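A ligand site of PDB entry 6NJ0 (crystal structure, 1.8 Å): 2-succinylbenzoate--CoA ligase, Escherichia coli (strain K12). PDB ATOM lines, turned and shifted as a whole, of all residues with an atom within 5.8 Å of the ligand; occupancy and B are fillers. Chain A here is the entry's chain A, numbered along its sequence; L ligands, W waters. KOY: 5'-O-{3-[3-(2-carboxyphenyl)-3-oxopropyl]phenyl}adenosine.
The side-chain carboxylate (OD1) of Asp 336 is in hydrogen-bond range of an oxygen (O7) of the ligand.
The side-chain hydroxyl of Thr 277 sits at hydrogen-bond distance from an oxygen (O2) of the ligand (2.7 Å).
The backbone carbonyl oxygen of Gly 268 lies within hydrogen-bond range of a nitrogen (N5) of the ligand, 2.8 Å away.
O1 of the ligand is in salt-bridge range of NH2 of Arg 195 (2.9 Å).
OD2 of Asp 336 is in hydrogen-bond range of OH of Tyr 269, 2.7 Å away.
The side-chain hydroxyl of Thr 334 sits at hydrogen-bond distance from the backbone NH of Asp 336 (2.9 Å).
NH2 of Arg 195 is in hydrogen-bond range of OG1 of Thr 277 (3.5 Å).
NH2 of Arg 195 sits at hydrogen-bond distance from OG of Ser 276 (2.9 Å).
NE of Arg 195 sits close to O of Gly 191 (3.3 Å).
The backbone carbonyl oxygen of Ser 276 is in hydrogen-bond range of the backbone NH of Leu 271, at 3.1 Å.
O of Leu 223 is in hydrogen-bond range of N of Gly 246, at 3.4 Å.
N of Leu 223 is in hydrogen-bond range of O of Leu 244, 2.9 Å away.
Residues that only touch the ligand: Leu 182, Val 187, Ser 188, Ser 222, Leu 223, Leu 244, Leu 245, Gly 246, Gly 247, Ala 248, Ala 249, Tyr 269, Gly 270, Leu 271, Thr 272, Ser 276, Val 289, Ile 347 and Arg 350.
Of the 32 residues printed, 23 come within 4 Å of the ligand.
Water W2 lies within hydrogen-bond range of O2 of the ligand (2.6 Å), O of Gly 268 (3.3 Å) and O of Leu 245 (3.5 Å).
Water W4 lies within hydrogen-bond range of an oxygen (O1) of the ligand, the side-chain hydroxyl of Ser 222, the guanidinium group of Arg 195 and the backbone carbonyl oxygen of Ser 188.
Water W1 lies within hydrogen-bond range of the backbone NH (N) of Gly 247 (2.9 Å), a nitrogen (N4) of the ligand (3.0 Å), the backbone NH (N) of Gly 270 (3.0 Å) and the backbone carbonyl oxygen (O) of Gly 268 (3.2 Å).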
ATOM      1  N   SER A 143       5.362   5.725  35.282  1.00  0.00           N
ATOM      2  CA  SER A 143       5.609   4.246  35.131  1.00  0.00           C
ATOM      3  C   SER A 143       5.681   3.779  33.676  1.00  0.00           C
ATOM      4  O   SER A 143       6.342   4.430  32.874  1.00  0.00           O
ATOM      5  CB  SER A 143       4.584   3.400  35.940  1.00  0.00           C
ATOM      6  OG  SER A 143       3.268   3.506  35.473  1.00  0.00           O
ATOM      7  N   VAL A 166     -12.772  16.674  30.965  1.00  0.00           N
ATOM      8  CA  VAL A 166     -13.357  15.382  30.678  1.00  0.00           C
ATOM      9  C   VAL A 166     -14.848  15.495  30.593  1.00  0.00           C
ATOM     10  O   VAL A 166     -15.416  14.967  29.668  1.00  0.00           O
ATOM     11  CB  VAL A 166     -13.004  14.290  31.648  1.00  0.00           C
ATOM     12  CG1 VAL A 166     -13.753  12.969  31.331  1.00  0.00           C
ATOM     13  CG2 VAL A 166     -11.499  14.049  31.595  1.00  0.00           C
ATOM     14  N   LEU A 182     -10.514   1.919  38.427  1.00  0.00           N
ATOM     15  CA  LEU A 182      -9.095   1.939  38.173  1.00  0.00           C
ATOM     16  C   LEU A 182      -8.395   2.569  39.401  1.00  0.00           C
ATOM     17  O   LEU A 182      -9.031   3.295  40.180  1.00  0.00           O
ATOM     18  CB  LEU A 182      -8.745   2.672  36.868  1.00  0.00           C
ATOM     19  CG  LEU A 182      -9.068   1.961  35.540  1.00  0.00           C
ATOM     20  CD1 LEU A 182      -8.793   2.922  34.391  1.00  0.00           C
ATOM     21  CD2 LEU A 182      -8.250   0.680  35.405  1.00  0.00           C
ATOM     22  N   VAL A 187      -3.459   8.129  37.857  1.00  0.00           N
ATOM     23  CA  VAL A 187      -4.285   9.353  37.592  1.00  0.00           C
ATOM     24  C   VAL A 187      -5.682   8.942  37.118  1.00  0.00           C
ATOM     25  O   VAL A 187      -6.586   9.681  37.228  1.00  0.00           O
ATOM     26  CB  VAL A 187      -3.625  10.418  36.707  1.00  0.00           C
ATOM     27  CG1 VAL A 187      -2.342  10.898  37.346  1.00  0.00           C
ATOM     28  CG2 VAL A 187      -3.342   9.915  35.304  1.00  0.00           C
ATOM     29  N   SER A 188      -5.804   7.778  36.530  1.00  0.00           N
ATOM     30  CA  SER A 188      -7.053   7.252  36.076  1.00  0.00           C
ATOM     31  C   SER A 188      -8.086   7.169  37.198  1.00  0.00           C
ATOM     32  O   SER A 188      -9.204   7.637  37.028  1.00  0.00           O
ATOM     33  CB  SER A 188      -6.823   5.860  35.387  1.00  0.00           C
ATOM     34  OG  SER A 188      -6.206   4.969  36.306  1.00  0.00           O
ATOM     35  N   GLY A 191      -8.848  10.585  38.557  1.00  0.00           N
ATOM     36  CA  GLY A 191      -9.709  11.334  37.683  1.00  0.00           C
ATOM     37  C   GLY A 191     -11.148  11.034  37.907  1.00  0.00           C
ATOM     38  O   GLY A 191     -11.995  11.924  37.843  1.00  0.00           O
ATOM     39  N   ARG A 195     -13.807  13.807  39.055  1.00  0.00           N
ATOM     40  CA  ARG A 195     -15.019  14.002  38.233  1.00  0.00           C
ATOM     41  C   ARG A 195     -16.287  13.926  39.059  1.00  0.00           C
ATOM     42  O   ARG A 195     -17.207  14.750  38.833  1.00  0.00           O
ATOM     43  CB  ARG A 195     -15.028  13.014  37.074  1.00  0.00           C
ATOM     44  CG  ARG A 195     -14.003  13.384  35.998  1.00  0.00           C
ATOM     45  CD  ARG A 195     -13.743  12.218  35.053  1.00  0.00           C
ATOM     46  NE  ARG A 195     -12.379  12.194  34.624  1.00  0.00           N
ATOM     47  CZ  ARG A 195     -11.694  11.112  34.259  1.00  0.00           C
ATOM     48  NH1 ARG A 195     -12.259   9.920  34.227  1.00  0.00           N
ATOM     49  NH2 ARG A 195     -10.400  11.247  33.989  1.00  0.00           N
ATOM     50  N   SER A 222     -14.361   3.838  33.989  1.00  0.00           N
ATOM     51  CA  SER A 222     -13.118   3.958  33.259  1.00  0.00           C
ATOM     52  C   SER A 222     -12.413   2.577  33.136  1.00  0.00           C
ATOM     53  O   SER A 222     -12.164   1.943  34.154  1.00  0.00           O
ATOM     54  CB  SER A 222     -12.185   4.877  33.986  1.00  0.00           C
ATOM     55  OG  SER A 222     -12.718   6.160  34.095  1.00  0.00           O
ATOM     56  N   LEU A 223     -12.044   2.195  31.914  1.00  0.00           N
ATOM     57  CA  LEU A 223     -11.445   0.889  31.688  1.00  0.00           C
ATOM     58  C   LEU A 223     -10.178   0.993  30.886  1.00  0.00           C
ATOM     59  O   LEU A 223     -10.011   1.827  30.013  1.00  0.00           O
ATOM     60  CB  LEU A 223     -12.497  -0.033  30.994  1.00  0.00           C
ATOM     61  CG  LEU A 223     -13.751  -0.338  31.842  1.00  0.00           C
ATOM     62  CD1 LEU A 223     -14.559  -1.370  31.086  1.00  0.00           C
ATOM     63  CD2 LEU A 223     -13.543  -0.900  33.269  1.00  0.00           C
ATOM     64  N   VAL A 224      -9.203   0.182  31.249  1.00  0.00           N
ATOM     65  CA  VAL A 224      -8.206  -0.224  30.298  1.00  0.00           C
ATOM     66  C   VAL A 224      -8.736  -1.267  29.331  1.00  0.00           C
ATOM     67  O   VAL A 224      -9.678  -2.031  29.645  1.00  0.00           O
ATOM     68  CB  VAL A 224      -6.909  -0.692  30.941  1.00  0.00           C
ATOM     69  CG1 VAL A 224      -6.267   0.468  31.755  1.00  0.00           C
ATOM     70  CG2 VAL A 224      -7.115  -1.894  31.807  1.00  0.00           C
ATOM     71  N   LEU A 244     -14.982   5.232  29.575  1.00  0.00           N
ATOM     72  CA  LEU A 244     -13.818   5.989  29.049  1.00  0.00           C
ATOM     73  C   LEU A 244     -12.626   5.032  29.063  1.00  0.00           C
ATOM     74  O   LEU A 244     -12.305   4.479  30.148  1.00  0.00           O
ATOM     75  CB  LEU A 244     -13.498   7.229  29.864  1.00  0.00           C
ATOM     76  CG  LEU A 244     -12.180   7.956  29.610  1.00  0.00           C
ATOM     77  CD1 LEU A 244     -12.161   8.532  28.188  1.00  0.00           C
ATOM     78  CD2 LEU A 244     -11.897   9.039  30.620  1.00  0.00           C
ATOM     79  N   LEU A 245     -12.027   4.844  27.896  1.00  0.00           N
ATOM     80  CA  LEU A 245     -10.851   3.986  27.752  1.00  0.00           C
ATOM     81  C   LEU A 245      -9.601   4.796  27.676  1.00  0.00           C
ATOM     82  O   LEU A 245      -9.585   5.908  27.181  1.00  0.00           O
ATOM     83  CB  LEU A 245     -10.987   3.093  26.531  1.00  0.00           C
ATOM     84  CG  LEU A 245     -12.190   2.158  26.449  1.00  0.00           C
ATOM     85  CD1 LEU A 245     -12.574   1.900  25.023  1.00  0.00           C
ATOM     86  CD2 LEU A 245     -11.834   0.838  27.147  1.00  0.00           C
ATOM     87  N   GLY A 246      -8.501   4.220  28.154  1.00  0.00           N
ATOM     88  CA  GLY A 246      -7.221   4.820  27.960  1.00  0.00           C
ATOM     89  C   GLY A 246      -6.084   3.920  28.381  1.00  0.00           C
ATOM     90  O   GLY A 246      -6.271   2.688  28.667  1.00  0.00           O
ATOM     91  N   GLY A 247      -4.925   4.574  28.483  1.00  0.00           N
ATOM     92  CA  GLY A 247      -3.708   3.946  28.988  1.00  0.00           C
ATOM     93  C   GLY A 247      -2.777   3.441  27.901  1.00  0.00           C
ATOM     94  O   GLY A 247      -1.637   3.092  28.201  1.00  0.00           O
ATOM     95  N   ALA A 248      -3.248   3.467  26.658  1.00  0.00           N
ATOM     96  CA  ALA A 248      -2.614   2.854  25.493  1.00  0.00           C
ATOM     97  C   ALA A 248      -3.538   3.178  24.286  1.00  0.00           C
ATOM     98  O   ALA A 248      -4.630   3.645  24.494  1.00  0.00           O
ATOM     99  CB  ALA A 248      -2.551   1.333  25.690  1.00  0.00           C
ATOM    100  N   ALA A 249      -3.096   2.929  23.056  1.00  0.00           N
ATOM    101  CA  ALA A 249      -3.969   2.970  21.862  1.00  0.00           C
ATOM    102  C   ALA A 249      -5.146   2.021  22.040  1.00  0.00           C
ATOM    103  O   ALA A 249      -5.027   0.987  22.683  1.00  0.00           O
ATOM    104  CB  ALA A 249      -3.216   2.521  20.623  1.00  0.00           C
ATOM    105  N   ILE A 250      -6.280   2.399  21.512  1.00  0.00           N
ATOM    106  CA  ILE A 250      -7.461   1.631  21.732  1.00  0.00           C
ATOM    107  C   ILE A 250      -7.866   1.058  20.382  1.00  0.00           C
ATOM    108  O   ILE A 250      -8.305   1.799  19.543  1.00  0.00           O
ATOM    109  CB  ILE A 250      -8.532   2.501  22.397  1.00  0.00           C
ATOM    110  CG1 ILE A 250      -8.101   2.903  23.803  1.00  0.00           C
ATOM    111  CG2 ILE A 250      -9.836   1.773  22.521  1.00  0.00           C
ATOM    112  CD1 ILE A 250      -8.137   4.409  23.981  1.00  0.00           C
ATOM    113  N   CYS A 267     -12.575   7.225  23.981  1.00  0.00           N
ATOM    114  CA  CYS A 267     -11.181   6.888  23.910  1.00  0.00           C
ATOM    115  C   CYS A 267     -10.374   8.101  24.283  1.00  0.00           C
ATOM    116  O   CYS A 267     -10.593   9.169  23.780  1.00  0.00           O
ATOM    117  CB  CYS A 267     -10.841   6.500  22.483  1.00  0.00           C
ATOM    118  SG  CYS A 267     -11.837   5.048  21.987  1.00  0.00           S
ATOM    119  N   GLY A 268      -9.424   7.948  25.179  1.00  0.00           N
ATOM    120  CA  GLY A 268      -8.622   9.087  25.623  1.00  0.00           C
ATOM    121  C   GLY A 268      -7.136   8.874  25.494  1.00  0.00           C
ATOM    122  O   GLY A 268      -6.681   7.767  25.443  1.00  0.00           O
ATOM    123  N   TYR A 269      -6.428   9.961  25.307  1.00  0.00           N
ATOM    124  CA  TYR A 269      -4.965  10.063  25.381  1.00  0.00           C
ATOM    125  C   TYR A 269      -4.720  10.891  26.603  1.00  0.00           C
ATOM    126  O   TYR A 269      -5.165  12.017  26.708  1.00  0.00           O
ATOM    127  CB  TYR A 269      -4.387  10.732  24.145  1.00  0.00           C
ATOM    128  CG  TYR A 269      -2.975  11.227  24.193  1.00  0.00           C
ATOM    129  CD1 TYR A 269      -1.918  10.345  24.352  1.00  0.00           C
ATOM    130  CD2 TYR A 269      -2.678  12.581  24.150  1.00  0.00           C
ATOM    131  CE1 TYR A 269      -0.605  10.817  24.435  1.00  0.00           C
ATOM    132  CE2 TYR A 269      -1.356  13.040  24.192  1.00  0.00           C
ATOM    133  CZ  TYR A 269      -0.336  12.163  24.345  1.00  0.00           C
ATOM    134  OH  TYR A 269       0.970  12.573  24.331  1.00  0.00           O
ATOM    135  N   GLY A 270      -4.037  10.307  27.573  1.00  0.00           N
ATOM    136  CA  GLY A 270      -3.794  11.017  28.822  1.00  0.00           C
ATOM    137  C   GLY A 270      -2.393  10.715  29.306  1.00  0.00           C
ATOM    138  O   GLY A 270      -1.662   9.955  28.697  1.00  0.00           O
ATOM    139  N   LEU A 271      -2.007  11.384  30.369  1.00  0.00           N
ATOM    140  CA  LEU A 271      -0.687  11.189  30.908  1.00  0.00           C
ATOM    141  C   LEU A 271      -0.734  11.386  32.434  1.00  0.00           C
ATOM    142  O   LEU A 271      -1.515  12.127  32.943  1.00  0.00           O
ATOM    143  CB  LEU A 271       0.287  12.231  30.323  1.00  0.00           C
ATOM    144  CG  LEU A 271       0.843  12.184  28.920  1.00  0.00           C
ATOM    145  CD1 LEU A 271      -0.259  12.637  27.959  1.00  0.00           C
ATOM    146  CD2 LEU A 271       2.001  13.175  28.787  1.00  0.00           C
ATOM    147  N   THR A 272       0.236  10.830  33.136  1.00  0.00           N
ATOM    148  CA  THR A 272       0.305  11.040  34.563  1.00  0.00           C
ATOM    149  C   THR A 272       0.478  12.520  34.885  1.00  0.00           C
ATOM    150  O   THR A 272      -0.078  13.053  35.847  1.00  0.00           O
ATOM    151  CB  THR A 272       1.532  10.304  35.114  1.00  0.00           C
ATOM    152  OG1 THR A 272       1.448   8.909  34.756  1.00  0.00           O
ATOM    153  CG2 THR A 272       1.632  10.496  36.634  1.00  0.00           C
ATOM    154  N   ALA A 275      -2.764  14.511  35.107  1.00  0.00           N
ATOM    155  CA  ALA A 275      -3.795  14.051  36.062  1.00  0.00           C
ATOM    156  C   ALA A 275      -4.956  13.405  35.296  1.00  0.00           C
ATOM    157  O   ALA A 275      -6.116  13.473  35.764  1.00  0.00           O
ATOM    158  CB  ALA A 275      -4.301  15.230  36.927  1.00  0.00           C
ATOM    159  N   SER A 276      -4.577  12.689  34.229  1.00  0.00           N
ATOM    160  CA  SER A 276      -5.479  11.883  33.358  1.00  0.00           C
ATOM    161  C   SER A 276      -5.608  12.464  31.942  1.00  0.00           C
ATOM    162  O   SER A 276      -4.603  12.769  31.318  1.00  0.00           O
ATOM    163  CB  SER A 276      -6.862  11.434  33.976  1.00  0.00           C
ATOM    164  OG  SER A 276      -7.783  12.476  34.030  1.00  0.00           O
ATOM    165  N   THR A 277      -6.829  12.698  31.445  1.00  0.00           N
ATOM    166  CA  THR A 277      -7.076  12.846  30.011  1.00  0.00           C
ATOM    167  C   THR A 277      -6.688  14.156  29.384  1.00  0.00           C
ATOM    168  O   THR A 277      -6.972  15.234  29.907  1.00  0.00           O
ATOM    169  CB  THR A 277      -8.604  12.630  29.725  1.00  0.00           C
ATOM    170  OG1 THR A 277      -9.167  11.790  30.779  1.00  0.00           O
ATOM    171  CG2 THR A 277      -8.777  11.969  28.390  1.00  0.00           C
ATOM    172  N   VAL A 289      -6.441  10.365  18.311  1.00  0.00           N
ATOM    173  CA  VAL A 289      -6.877  10.286  19.717  1.00  0.00           C
ATOM    174  C   VAL A 289      -7.835  11.375  20.069  1.00  0.00           C
ATOM    175  O   VAL A 289      -8.120  11.638  21.246  1.00  0.00           O
ATOM    176  CB  VAL A 289      -5.681  10.311  20.691  1.00  0.00           C
ATOM    177  CG1 VAL A 289      -4.821   9.070  20.466  1.00  0.00           C
ATOM    178  CG2 VAL A 289      -4.884  11.595  20.513  1.00  0.00           C
ATOM    179  N   THR A 334       6.415  15.707  25.641  1.00  0.00           N
ATOM    180  CA  THR A 334       5.947  14.369  26.007  1.00  0.00           C
ATOM    181  C   THR A 334       6.862  13.225  25.667  1.00  0.00           C
ATOM    182  O   THR A 334       6.650  12.130  26.164  1.00  0.00           O
ATOM    183  CB  THR A 334       4.607  14.015  25.288  1.00  0.00           C
ATOM    184  OG1 THR A 334       4.818  14.021  23.871  1.00  0.00           O
ATOM    185  CG2 THR A 334       3.500  14.976  25.653  1.00  0.00           C
ATOM    186  N   ASP A 336       6.399  11.759  22.959  1.00  0.00           N
ATOM    187  CA  ASP A 336       5.544  11.065  22.029  1.00  0.00           C
ATOM    188  C   ASP A 336       5.744  11.768  20.664  1.00  0.00           C
ATOM    189  O   ASP A 336       5.911  12.987  20.597  1.00  0.00           O
ATOM    190  CB  ASP A 336       4.075  11.165  22.412  1.00  0.00           C
ATOM    191  CG  ASP A 336       3.654  10.196  23.561  1.00  0.00           C
ATOM    192  OD1 ASP A 336       4.256   9.112  23.643  1.00  0.00           O
ATOM    193  OD2 ASP A 336       2.746  10.578  24.386  1.00  0.00           O
ATOM    194  N   ILE A 347      -1.200   9.976  17.439  1.00  0.00           N
ATOM    195  CA  ILE A 347       0.058   9.511  18.007  1.00  0.00           C
ATOM    196  C   ILE A 347       0.681   8.539  16.996  1.00  0.00           C
ATOM    197  O   ILE A 347       0.117   7.496  16.702  1.00  0.00           O
ATOM    198  CB  ILE A 347      -0.184   8.851  19.369  1.00  0.00           C
ATOM    199  CG1 ILE A 347      -0.840   9.869  20.353  1.00  0.00           C
ATOM    200  CG2 ILE A 347       1.118   8.237  19.921  1.00  0.00           C
ATOM    201  CD1 ILE A 347       0.024  11.106  20.544  1.00  0.00           C
ATOM    202  N   GLY A 349       4.074   7.383  17.485  1.00  0.00           N
ATOM    203  CA  GLY A 349       4.902   6.506  18.267  1.00  0.00           C
ATOM    204  C   GLY A 349       5.636   7.175  19.385  1.00  0.00           C
ATOM    205  O   GLY A 349       5.298   8.258  19.704  1.00  0.00           O
ATOM    206  N   ARG A 350       6.616   6.499  19.970  1.00  0.00           N
ATOM    207  CA  ARG A 350       7.421   7.055  21.042  1.00  0.00           C
ATOM    208  C   ARG A 350       8.793   7.415  20.570  1.00  0.00           C
ATOM    209  O   ARG A 350       9.453   6.606  20.047  1.00  0.00           O
ATOM    210  CB  ARG A 350       7.589   6.080  22.189  1.00  0.00           C
ATOM    211  CG  ARG A 350       6.452   6.028  23.165  1.00  0.00           C
ATOM    212  CD  ARG A 350       6.272   4.630  23.701  1.00  0.00           C
ATOM    213  NE  ARG A 350       6.021   4.639  25.147  1.00  0.00           N
ATOM    214  CZ  ARG A 350       4.871   4.280  25.714  1.00  0.00           C
ATOM    215  NH1 ARG A 350       3.835   3.886  24.981  1.00  0.00           N
ATOM    216  NH2 ARG A 350       4.765   4.345  27.015  1.00  0.00           N
HETATM  217  C1  KOY L   1      -1.484   6.406  23.945  1.00  0.00           C
HETATM  218  C2  KOY L   1      -2.808   6.706  24.166  1.00  0.00           C
HETATM  219  C3  KOY L   1      -3.685   6.738  23.132  1.00  0.00           C
HETATM  220  C4  KOY L   1      -1.708   6.729  26.034  1.00  0.00           C
HETATM  221  N1  KOY L   1      -3.265   6.492  21.868  1.00  0.00           N
HETATM  222  N2  KOY L   1      -1.030   6.148  22.701  1.00  0.00           N
HETATM  223  O1  KOY L   1      -9.014   8.979  32.808  1.00  0.00           O
HETATM  224  C5  KOY L   1      -8.488   8.512  31.766  1.00  0.00           C
HETATM  225  O2  KOY L   1      -8.227   9.298  30.827  1.00  0.00           O
HETATM  226  C6  KOY L   1      -8.206   7.104  31.657  1.00  0.00           C
HETATM  227  C7  KOY L   1      -9.283   6.233  31.525  1.00  0.00           C
HETATM  228  C8  KOY L   1      -9.094   4.844  31.458  1.00  0.00           C
HETATM  229  C9  KOY L   1      -7.843   4.309  31.563  1.00  0.00           C
HETATM  230  C10 KOY L   1      -6.741   5.182  31.656  1.00  0.00           C
HETATM  231  C11 KOY L   1      -6.887   6.579  31.812  1.00  0.00           C
HETATM  232  C12 KOY L   1      -5.766   7.457  31.974  1.00  0.00           C
HETATM  233  O3  KOY L   1      -5.849   8.525  32.596  1.00  0.00           O
HETATM  234  C13 KOY L   1      -4.329   6.972  31.730  1.00  0.00           C
HETATM  235  C14 KOY L   1      -3.290   8.118  31.733  1.00  0.00           C
HETATM  236  C15 KOY L   1      -1.961   7.619  31.552  1.00  0.00           C
HETATM  237  C16 KOY L   1      -1.503   7.306  30.274  1.00  0.00           C
HETATM  238  C17 KOY L   1      -1.056   7.468  32.624  1.00  0.00           C
HETATM  239  C18 KOY L   1       0.190   6.946  32.404  1.00  0.00           C
HETATM  240  C19 KOY L   1       0.624   6.632  31.121  1.00  0.00           C
HETATM  241  C20 KOY L   1      -0.216   6.804  30.032  1.00  0.00           C
HETATM  242  O4  KOY L   1       0.159   6.549  28.723  1.00  0.00           O
HETATM  243  C21 KOY L   1       1.522   6.903  28.418  1.00  0.00           C
HETATM  244  C22 KOY L   1       1.881   6.698  26.937  1.00  0.00           C
HETATM  245  O5  KOY L   1       1.101   5.671  26.430  1.00  0.00           O
HETATM  246  C23 KOY L   1       1.574   7.994  26.181  1.00  0.00           C
HETATM  247  O6  KOY L   1       2.613   8.977  26.384  1.00  0.00           O
HETATM  248  C24 KOY L   1       1.519   7.459  24.807  1.00  0.00           C
HETATM  249  O7  KOY L   1       2.927   7.206  24.253  1.00  0.00           O
HETATM  250  C25 KOY L   1       0.684   6.143  25.116  1.00  0.00           C
HETATM  251  N3  KOY L   1      -0.804   6.451  25.099  1.00  0.00           N
HETATM  252  N4  KOY L   1      -2.931   6.896  25.477  1.00  0.00           N
HETATM  253  C26 KOY L   1      -1.960   6.184  21.621  1.00  0.00           C
HETATM  254  N5  KOY L   1      -4.972   7.032  23.358  1.00  0.00           N
HETATM  255  O   HOH W   1      -4.596   7.393  27.885  1.00  0.00           O
HETATM  256  O   HOH W   2      -7.366   8.192  28.608  1.00  0.00           O
HETATM  257  O   HOH W   3      -3.419   6.183  34.952  1.00  0.00           O
HETATM  258  O   HOH W   4     -10.555   7.678  34.503  1.00  0.00           O
